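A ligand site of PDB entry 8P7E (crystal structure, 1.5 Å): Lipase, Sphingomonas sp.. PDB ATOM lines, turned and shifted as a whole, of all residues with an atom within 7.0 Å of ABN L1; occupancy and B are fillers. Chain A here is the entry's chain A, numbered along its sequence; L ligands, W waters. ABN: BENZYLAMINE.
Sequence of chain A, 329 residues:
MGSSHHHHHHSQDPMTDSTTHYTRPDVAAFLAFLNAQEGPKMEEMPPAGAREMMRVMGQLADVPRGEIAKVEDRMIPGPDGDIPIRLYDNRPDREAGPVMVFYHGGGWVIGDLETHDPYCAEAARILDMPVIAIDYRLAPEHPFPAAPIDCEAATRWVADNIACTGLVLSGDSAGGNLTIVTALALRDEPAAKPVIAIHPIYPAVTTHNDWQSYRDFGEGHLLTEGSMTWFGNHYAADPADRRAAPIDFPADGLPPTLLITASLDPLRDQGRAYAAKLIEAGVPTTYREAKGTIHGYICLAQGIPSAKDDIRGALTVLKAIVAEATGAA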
ATOM      1  N   GLY A 105      18.865 -11.509  -3.783  1.00  0.00           N
ATOM      2  CA  GLY A 105      18.990 -12.621  -4.687  1.00  0.00           C
ATOM      3  C   GLY A 105      18.699 -12.242  -6.146  1.00  0.00           C
ATOM      4  O   GLY A 105      18.471 -11.084  -6.482  1.00  0.00           O
ATOM      5  N   GLY A 106      18.750 -13.266  -6.986  1.00  0.00           N
ATOM      6  CA  GLY A 106      18.678 -13.061  -8.421  1.00  0.00           C
ATOM      7  C   GLY A 106      19.748 -13.859  -9.162  1.00  0.00           C
ATOM      8  O   GLY A 106      20.135 -13.459 -10.276  1.00  0.00           O
ATOM      9  N   GLY A 107      20.246 -14.956  -8.627  1.00  0.00           N
ATOM     10  CA  GLY A 107      21.136 -15.853  -9.351  1.00  0.00           C
ATOM     11  C   GLY A 107      22.424 -15.184  -9.764  1.00  0.00           C
ATOM     12  O   GLY A 107      23.069 -15.647 -10.727  1.00  0.00           O
ATOM     13  N   TRP A 108      22.837 -14.126  -9.058  1.00  0.00           N
ATOM     14  CA  TRP A 108      24.056 -13.374  -9.306  1.00  0.00           C
ATOM     15  C   TRP A 108      23.998 -12.634 -10.652  1.00  0.00           C
ATOM     16  O   TRP A 108      25.025 -12.066 -11.029  1.00  0.00           O
ATOM     17  CB  TRP A 108      25.298 -14.245  -9.191  1.00  0.00           C
ATOM     18  CG  TRP A 108      25.424 -15.014  -7.918  1.00  0.00           C
ATOM     19  CD1 TRP A 108      25.908 -14.544  -6.730  1.00  0.00           C
ATOM     20  CD2 TRP A 108      25.052 -16.373  -7.695  1.00  0.00           C
ATOM     21  NE1 TRP A 108      25.883 -15.546  -5.784  1.00  0.00           N
ATOM     22  CE2 TRP A 108      25.328 -16.670  -6.333  1.00  0.00           C
ATOM     23  CE3 TRP A 108      24.502 -17.380  -8.481  1.00  0.00           C
ATOM     24  CZ2 TRP A 108      25.104 -17.940  -5.789  1.00  0.00           C
ATOM     25  CZ3 TRP A 108      24.251 -18.640  -7.940  1.00  0.00           C
ATOM     26  CH2 TRP A 108      24.534 -18.890  -6.599  1.00  0.00           C
ATOM     27  N   ASP A 172      18.707 -13.457   0.354  1.00  0.00           N
ATOM     28  CA  ASP A 172      17.916 -14.551  -0.187  1.00  0.00           C
ATOM     29  C   ASP A 172      18.605 -15.188  -1.384  1.00  0.00           C
ATOM     30  O   ASP A 172      19.058 -14.479  -2.274  1.00  0.00           O
ATOM     31  CB  ASP A 172      16.546 -14.021  -0.604  1.00  0.00           C
ATOM     32  CG  ASP A 172      16.611 -12.925  -1.670  1.00  0.00           C
ATOM     33  OD1 ASP A 172      17.267 -11.907  -1.410  1.00  0.00           O
ATOM     34  OD2 ASP A 172      16.027 -13.127  -2.765  1.00  0.00           O
ATOM     35  N   SER A 173      18.616 -16.512  -1.426  1.00  0.00           N
ATOM     36  CA  SER A 173      19.031 -17.286  -2.602  1.00  0.00           C
ATOM     37  C   SER A 173      20.530 -17.053  -2.866  1.00  0.00           C
ATOM     38  O   SER A 173      21.377 -17.399  -2.053  1.00  0.00           O
ATOM     39  CB  SER A 173      18.064 -17.021  -3.692  1.00  0.00           C
ATOM     40  OG  SER A 173      18.275 -17.944  -4.774  1.00  0.00           O
ATOM     41  N   ALA A 174      20.907 -16.415  -3.992  1.00  0.00           N
ATOM     42  CA  ALA A 174      22.272 -15.980  -4.211  1.00  0.00           C
ATOM     43  C   ALA A 174      22.733 -15.082  -3.073  1.00  0.00           C
ATOM     44  O   ALA A 174      23.869 -15.098  -2.653  1.00  0.00           O
ATOM     45  CB  ALA A 174      22.356 -15.214  -5.511  1.00  0.00           C
ATOM     46  N   GLY A 175      21.820 -14.291  -2.526  1.00  0.00           N
ATOM     47  CA  GLY A 175      22.108 -13.444  -1.392  1.00  0.00           C
ATOM     48  C   GLY A 175      22.262 -14.184  -0.078  1.00  0.00           C
ATOM     49  O   GLY A 175      22.971 -13.704   0.813  1.00  0.00           O
ATOM     50  N   ASN A 177      23.677 -17.256  -0.117  1.00  0.00           N
ATOM     51  CA  ASN A 177      25.045 -17.656  -0.360  1.00  0.00           C
ATOM     52  C   ASN A 177      26.017 -16.547   0.084  1.00  0.00           C
ATOM     53  O   ASN A 177      26.931 -16.781   0.845  1.00  0.00           O
ATOM     54  CB  ASN A 177      25.167 -17.973  -1.855  1.00  0.00           C
ATOM     55  CG  ASN A 177      26.567 -18.303  -2.277  1.00  0.00           C
ATOM     56  OD1 ASN A 177      26.960 -19.498  -2.223  1.00  0.00           O
ATOM     57  ND2 ASN A 177      27.185 -17.290  -2.802  1.00  0.00           N
ATOM     58  N   TYR A 202      16.657 -19.279   2.059  1.00  0.00           N
ATOM     59  CA  TYR A 202      16.751 -20.313   1.006  1.00  0.00           C
ATOM     60  C   TYR A 202      18.050 -20.214   0.241  1.00  0.00           C
ATOM     61  O   TYR A 202      18.079 -19.987  -0.989  1.00  0.00           O
ATOM     62  CB  TYR A 202      15.466 -20.357   0.144  1.00  0.00           C
ATOM     63  CG  TYR A 202      14.780 -19.093  -0.243  1.00  0.00           C
ATOM     64  CD1 TYR A 202      15.253 -18.243  -1.195  1.00  0.00           C
ATOM     65  CD2 TYR A 202      13.557 -18.771   0.318  1.00  0.00           C
ATOM     66  CE1 TYR A 202      14.580 -17.101  -1.575  1.00  0.00           C
ATOM     67  CE2 TYR A 202      12.870 -17.635  -0.036  1.00  0.00           C
ATOM     68  CZ  TYR A 202      13.362 -16.795  -0.992  1.00  0.00           C
ATOM     69  OH  TYR A 202      12.686 -15.650  -1.342  1.00  0.00           O
ATOM     70  N   PRO A 203      19.195 -20.334   0.939  1.00  0.00           N
ATOM     71  CA  PRO A 203      20.491 -20.114   0.307  1.00  0.00           C
ATOM     72  C   PRO A 203      20.943 -21.245  -0.620  1.00  0.00           C
ATOM     73  O   PRO A 203      20.584 -22.394  -0.443  1.00  0.00           O
ATOM     74  CB  PRO A 203      21.456 -20.101   1.483  1.00  0.00           C
ATOM     75  CG  PRO A 203      20.810 -21.003   2.486  1.00  0.00           C
ATOM     76  CD  PRO A 203      19.336 -20.715   2.372  1.00  0.00           C
ATOM     77  N   ALA A 204      21.792 -20.878  -1.569  1.00  0.00           N
ATOM     78  CA  ALA A 204      22.655 -21.828  -2.253  1.00  0.00           C
ATOM     79  C   ALA A 204      23.964 -21.946  -1.514  1.00  0.00           C
ATOM     80  O   ALA A 204      24.547 -20.918  -1.148  1.00  0.00           O
ATOM     81  CB  ALA A 204      22.886 -21.334  -3.661  1.00  0.00           C
ATOM     82  N   THR A 206      26.315 -24.793  -2.386  1.00  0.00           N
ATOM     83  CA  THR A 206      27.188 -25.647  -3.190  1.00  0.00           C
ATOM     84  C   THR A 206      26.723 -25.536  -4.604  1.00  0.00           C
ATOM     85  O   THR A 206      25.563 -25.253  -4.879  1.00  0.00           O
ATOM     86  CB  THR A 206      27.146 -27.096  -2.695  1.00  0.00           C
ATOM     87  OG1 THR A 206      28.063 -27.836  -3.544  1.00  0.00           O
ATOM     88  CG2 THR A 206      25.783 -27.723  -2.740  1.00  0.00           C
ATOM     89  N   THR A 207      27.639 -25.888  -5.546  1.00  0.00           N
ATOM     90  CA  THR A 207      27.241 -25.969  -6.947  1.00  0.00           C
ATOM     91  C   THR A 207      26.654 -27.322  -7.324  1.00  0.00           C
ATOM     92  O   THR A 207      26.114 -27.415  -8.422  1.00  0.00           O
ATOM     93  CB  THR A 207      28.431 -25.645  -7.878  1.00  0.00           C
ATOM     94  OG1 THR A 207      29.398 -26.699  -7.791  1.00  0.00           O
ATOM     95  CG2 THR A 207      29.034 -24.312  -7.554  1.00  0.00           C
ATOM     96  N   ASN A 209      24.189 -30.647  -7.610  1.00  0.00           N
ATOM     97  CA  ASN A 209      22.747 -30.844  -7.680  1.00  0.00           C
ATOM     98  C   ASN A 209      22.314 -32.238  -7.254  1.00  0.00           C
ATOM     99  O   ASN A 209      21.183 -32.600  -7.530  1.00  0.00           O
ATOM    100  CB  ASN A 209      22.209 -30.560  -9.076  1.00  0.00           C
ATOM    101  CG  ASN A 209      22.447 -29.129  -9.491  1.00  0.00           C
ATOM    102  OD1 ASN A 209      22.351 -28.236  -8.646  1.00  0.00           O
ATOM    103  ND2 ASN A 209      22.824 -28.945 -10.749  1.00  0.00           N
ATOM    104  N   LEU A 223      12.026 -21.668  -9.499  1.00  0.00           N
ATOM    105  CA  LEU A 223      13.438 -21.906  -9.707  1.00  0.00           C
ATOM    106  C   LEU A 223      13.572 -23.281 -10.340  1.00  0.00           C
ATOM    107  O   LEU A 223      13.402 -24.321  -9.706  1.00  0.00           O
ATOM    108  CB  LEU A 223      14.196 -21.891  -8.372  1.00  0.00           C
ATOM    109  CG  LEU A 223      15.720 -22.023  -8.444  1.00  0.00           C
ATOM    110  CD1 LEU A 223      16.376 -20.868  -9.195  1.00  0.00           C
ATOM    111  CD2 LEU A 223      16.322 -22.145  -7.044  1.00  0.00           C
ATOM    112  N   THR A 224      13.937 -23.292 -11.620  1.00  0.00           N
ATOM    113  CA  THR A 224      13.966 -24.527 -12.367  1.00  0.00           C
ATOM    114  C   THR A 224      15.382 -24.927 -12.720  1.00  0.00           C
ATOM    115  O   THR A 224      16.316 -24.112 -12.647  1.00  0.00           O
ATOM    116  CB  THR A 224      13.161 -24.349 -13.640  1.00  0.00           C
ATOM    117  OG1 THR A 224      13.812 -23.372 -14.474  1.00  0.00           O
ATOM    118  CG2 THR A 224      11.753 -23.902 -13.361  1.00  0.00           C
ATOM    119  N   SER A 227      16.644 -22.446 -15.287  1.00  0.00           N
ATOM    120  CA  SER A 227      17.041 -21.130 -14.819  1.00  0.00           C
ATOM    121  C   SER A 227      18.353 -21.250 -14.056  1.00  0.00           C
ATOM    122  O   SER A 227      19.217 -20.395 -14.177  1.00  0.00           O
ATOM    123  CB  SER A 227      15.966 -20.462 -14.028  1.00  0.00           C
ATOM    124  OG  SER A 227      15.727 -21.081 -12.797  1.00  0.00           O
ATOM    125  N   MET A 228      18.508 -22.318 -13.255  1.00  0.00           N
ATOM    126  CA  MET A 228      19.725 -22.516 -12.471  1.00  0.00           C
ATOM    127  C   MET A 228      20.937 -22.679 -13.403  1.00  0.00           C
ATOM    128  O   MET A 228      21.958 -22.071 -13.172  1.00  0.00           O
ATOM    129  CB  MET A 228      19.608 -23.715 -11.528  1.00  0.00           C
ATOM    130  CG  MET A 228      18.682 -23.399 -10.361  1.00  0.00           C
ATOM    131  SD  MET A 228      18.485 -24.828  -9.245  1.00  0.00           S
ATOM    132  CE  MET A 228      17.135 -25.696  -9.964  1.00  0.00           C
ATOM    133  N   THR A 229      20.767 -23.414 -14.513  1.00  0.00           N
ATOM    134  CA  THR A 229      21.857 -23.551 -15.485  1.00  0.00           C
ATOM    135  C   THR A 229      22.242 -22.188 -16.082  1.00  0.00           C
ATOM    136  O   THR A 229      23.419 -21.862 -16.208  1.00  0.00           O
ATOM    137  CB  THR A 229      21.435 -24.517 -16.601  1.00  0.00           C
ATOM    138  OG1 THR A 229      21.283 -25.801 -16.014  1.00  0.00           O
ATOM    139  CG2 THR A 229      22.476 -24.642 -17.678  1.00  0.00           C
ATOM    140  N   TRP A 230      21.221 -21.407 -16.432  1.00  0.00           N
ATOM    141  CA  TRP A 230      21.395 -20.106 -17.066  1.00  0.00           C
ATOM    142  C   TRP A 230      22.145 -19.139 -16.136  1.00  0.00           C
ATOM    143  O   TRP A 230      23.159 -18.518 -16.490  1.00  0.00           O
ATOM    144  CB  TRP A 230      20.042 -19.561 -17.459  1.00  0.00           C
ATOM    145  CG  TRP A 230      20.019 -18.252 -18.199  1.00  0.00           C
ATOM    146  CD1 TRP A 230      20.019 -18.072 -19.563  1.00  0.00           C
ATOM    147  CD2 TRP A 230      19.901 -16.945 -17.646  1.00  0.00           C
ATOM    148  NE1 TRP A 230      19.895 -16.750 -19.851  1.00  0.00           N
ATOM    149  CE2 TRP A 230      19.821 -16.014 -18.697  1.00  0.00           C
ATOM    150  CE3 TRP A 230      19.839 -16.434 -16.347  1.00  0.00           C
ATOM    151  CZ2 TRP A 230      19.692 -14.636 -18.499  1.00  0.00           C
ATOM    152  CZ3 TRP A 230      19.739 -15.080 -16.146  1.00  0.00           C
ATOM    153  CH2 TRP A 230      19.651 -14.172 -17.203  1.00  0.00           C
ATOM    154  N   PHE A 231      21.693 -19.083 -14.873  1.00  0.00           N
ATOM    155  CA  PHE A 231      22.385 -18.247 -13.899  1.00  0.00           C
ATOM    156  C   PHE A 231      23.828 -18.696 -13.752  1.00  0.00           C
ATOM    157  O   PHE A 231      24.757 -17.864 -13.648  1.00  0.00           O
ATOM    158  CB  PHE A 231      21.665 -18.350 -12.552  1.00  0.00           C
ATOM    159  CG  PHE A 231      20.358 -17.628 -12.429  1.00  0.00           C
ATOM    160  CD1 PHE A 231      20.215 -16.302 -12.780  1.00  0.00           C
ATOM    161  CD2 PHE A 231      19.266 -18.267 -11.856  1.00  0.00           C
ATOM    162  CE1 PHE A 231      19.018 -15.631 -12.606  1.00  0.00           C
ATOM    163  CE2 PHE A 231      18.059 -17.600 -11.672  1.00  0.00           C
ATOM    164  CZ  PHE A 231      17.946 -16.270 -12.010  1.00  0.00           C
ATOM    165  N   GLY A 232      24.044 -20.002 -13.520  1.00  0.00           N
ATOM    166  CA  GLY A 232      25.343 -20.503 -13.215  1.00  0.00           C
ATOM    167  C   GLY A 232      26.338 -20.309 -14.369  1.00  0.00           C
ATOM    168  O   GLY A 232      27.482 -19.975 -14.143  1.00  0.00           O
ATOM    169  N   LEU A 267      16.614 -26.125  -3.745  1.00  0.00           N
ATOM    170  CA  LEU A 267      17.730 -25.849  -2.835  1.00  0.00           C
ATOM    171  C   LEU A 267      17.428 -26.259  -1.393  1.00  0.00           C
ATOM    172  O   LEU A 267      18.281 -26.089  -0.539  1.00  0.00           O
ATOM    173  CB  LEU A 267      18.065 -24.350  -2.841  1.00  0.00           C
ATOM    174  CG  LEU A 267      18.325 -23.699  -4.187  1.00  0.00           C
ATOM    175  CD1 LEU A 267      18.853 -22.291  -3.987  1.00  0.00           C
ATOM    176  CD2 LEU A 267      19.274 -24.529  -5.019  1.00  0.00           C
ATOM    177  N   GLN A 270      20.059 -28.755   0.426  1.00  0.00           N
ATOM    178  CA  GLN A 270      21.383 -28.203   0.737  1.00  0.00           C
ATOM    179  C   GLN A 270      21.287 -27.190   1.900  1.00  0.00           C
ATOM    180  O   GLN A 270      22.271 -27.014   2.664  1.00  0.00           O
ATOM    181  CB  GLN A 270      22.071 -27.655  -0.505  1.00  0.00           C
ATOM    182  CG  GLN A 270      21.494 -26.380  -1.070  1.00  0.00           C
ATOM    183  CD  GLN A 270      22.163 -26.080  -2.379  1.00  0.00           C
ATOM    184  OE1 GLN A 270      23.060 -25.235  -2.435  1.00  0.00           O
ATOM    185  NE2 GLN A 270      21.769 -26.759  -3.438  1.00  0.00           N
ATOM    186  N   HIS A 295      10.667 -21.472  -3.520  1.00  0.00           N
ATOM    187  CA  HIS A 295      11.780 -20.546  -3.625  1.00  0.00           C
ATOM    188  C   HIS A 295      11.274 -19.195  -4.109  1.00  0.00           C
ATOM    189  O   HIS A 295      10.415 -19.102  -4.995  1.00  0.00           O
ATOM    190  CB  HIS A 295      12.775 -21.066  -4.672  1.00  0.00           C
ATOM    191  CG  HIS A 295      14.117 -20.362  -4.638  1.00  0.00           C
ATOM    192  ND1 HIS A 295      15.066 -20.813  -3.766  1.00  0.00           N
ATOM    193  CD2 HIS A 295      14.623 -19.332  -5.291  1.00  0.00           C
ATOM    194  CE1 HIS A 295      16.138 -20.011  -3.923  1.00  0.00           C
ATOM    195  NE2 HIS A 295      15.898 -19.113  -4.817  1.00  0.00           N
HETATM  196  N   ABN L   1      20.821 -18.422  -6.768  1.00  0.00           N
HETATM  197  C   ABN L   1      19.875 -19.194  -7.571  1.00  0.00           C
HETATM  198  C1  ABN L   1      20.638 -20.386  -8.076  1.00  0.00           C
HETATM  199  C2  ABN L   1      20.843 -21.519  -7.317  1.00  0.00           C
HETATM  200  C3  ABN L   1      21.563 -22.598  -7.801  1.00  0.00           C
HETATM  201  C4  ABN L   1      22.100 -22.538  -9.063  1.00  0.00           C
HETATM  202  C5  ABN L   1      21.939 -21.400  -9.795  1.00  0.00           C
HETATM  203  C6  ABN L   1      21.211 -20.327  -9.331  1.00  0.00           C
HETATM  204  N   ABN L   2      25.827 -23.342 -10.278  1.00  0.00           N
HETATM  205  C   ABN L   2      25.720 -21.962  -9.764  1.00  0.00           C
HETATM  206  C1  ABN L   2      26.205 -21.773  -8.351  1.00  0.00           C
HETATM  207  C2  ABN L   2      27.248 -20.919  -8.082  1.00  0.00           C
HETATM  208  C3  ABN L   2      27.675 -20.689  -6.795  1.00  0.00           C
HETATM  209  C4  ABN L   2      27.121 -21.347  -5.763  1.00  0.00           C
HETATM  210  C5  ABN L   2      26.082 -22.191  -5.983  1.00  0.00           C
HETATM  211  C6  ABN L   2      25.612 -22.409  -7.259  1.00  0.00           C
HETATM  212  O   HOH W   1      19.214 -16.017  -6.292  1.00  0.00           O
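Merely in contact with ABN L1: Gly 107, Trp 108, Met 228, Phe 231 and Leu 267. Hydrophobic or aromatic side chains that line ABN L1: Trp 108, Ala 174, Met 228, Phe 231 and Leu 267.
OG of Ser 173 lies within hydrogen-bond range of NE2 of His 295, 2.6 Å away.
A nitrogen (N) of ABN L1 lies close to the backbone NH of Ala 174, at 3.4 Å. The side-chain hydroxyl of Ser 173 is in hydrogen-bond range of a nitrogen (N) of ABN L1, at 3.3 Å.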
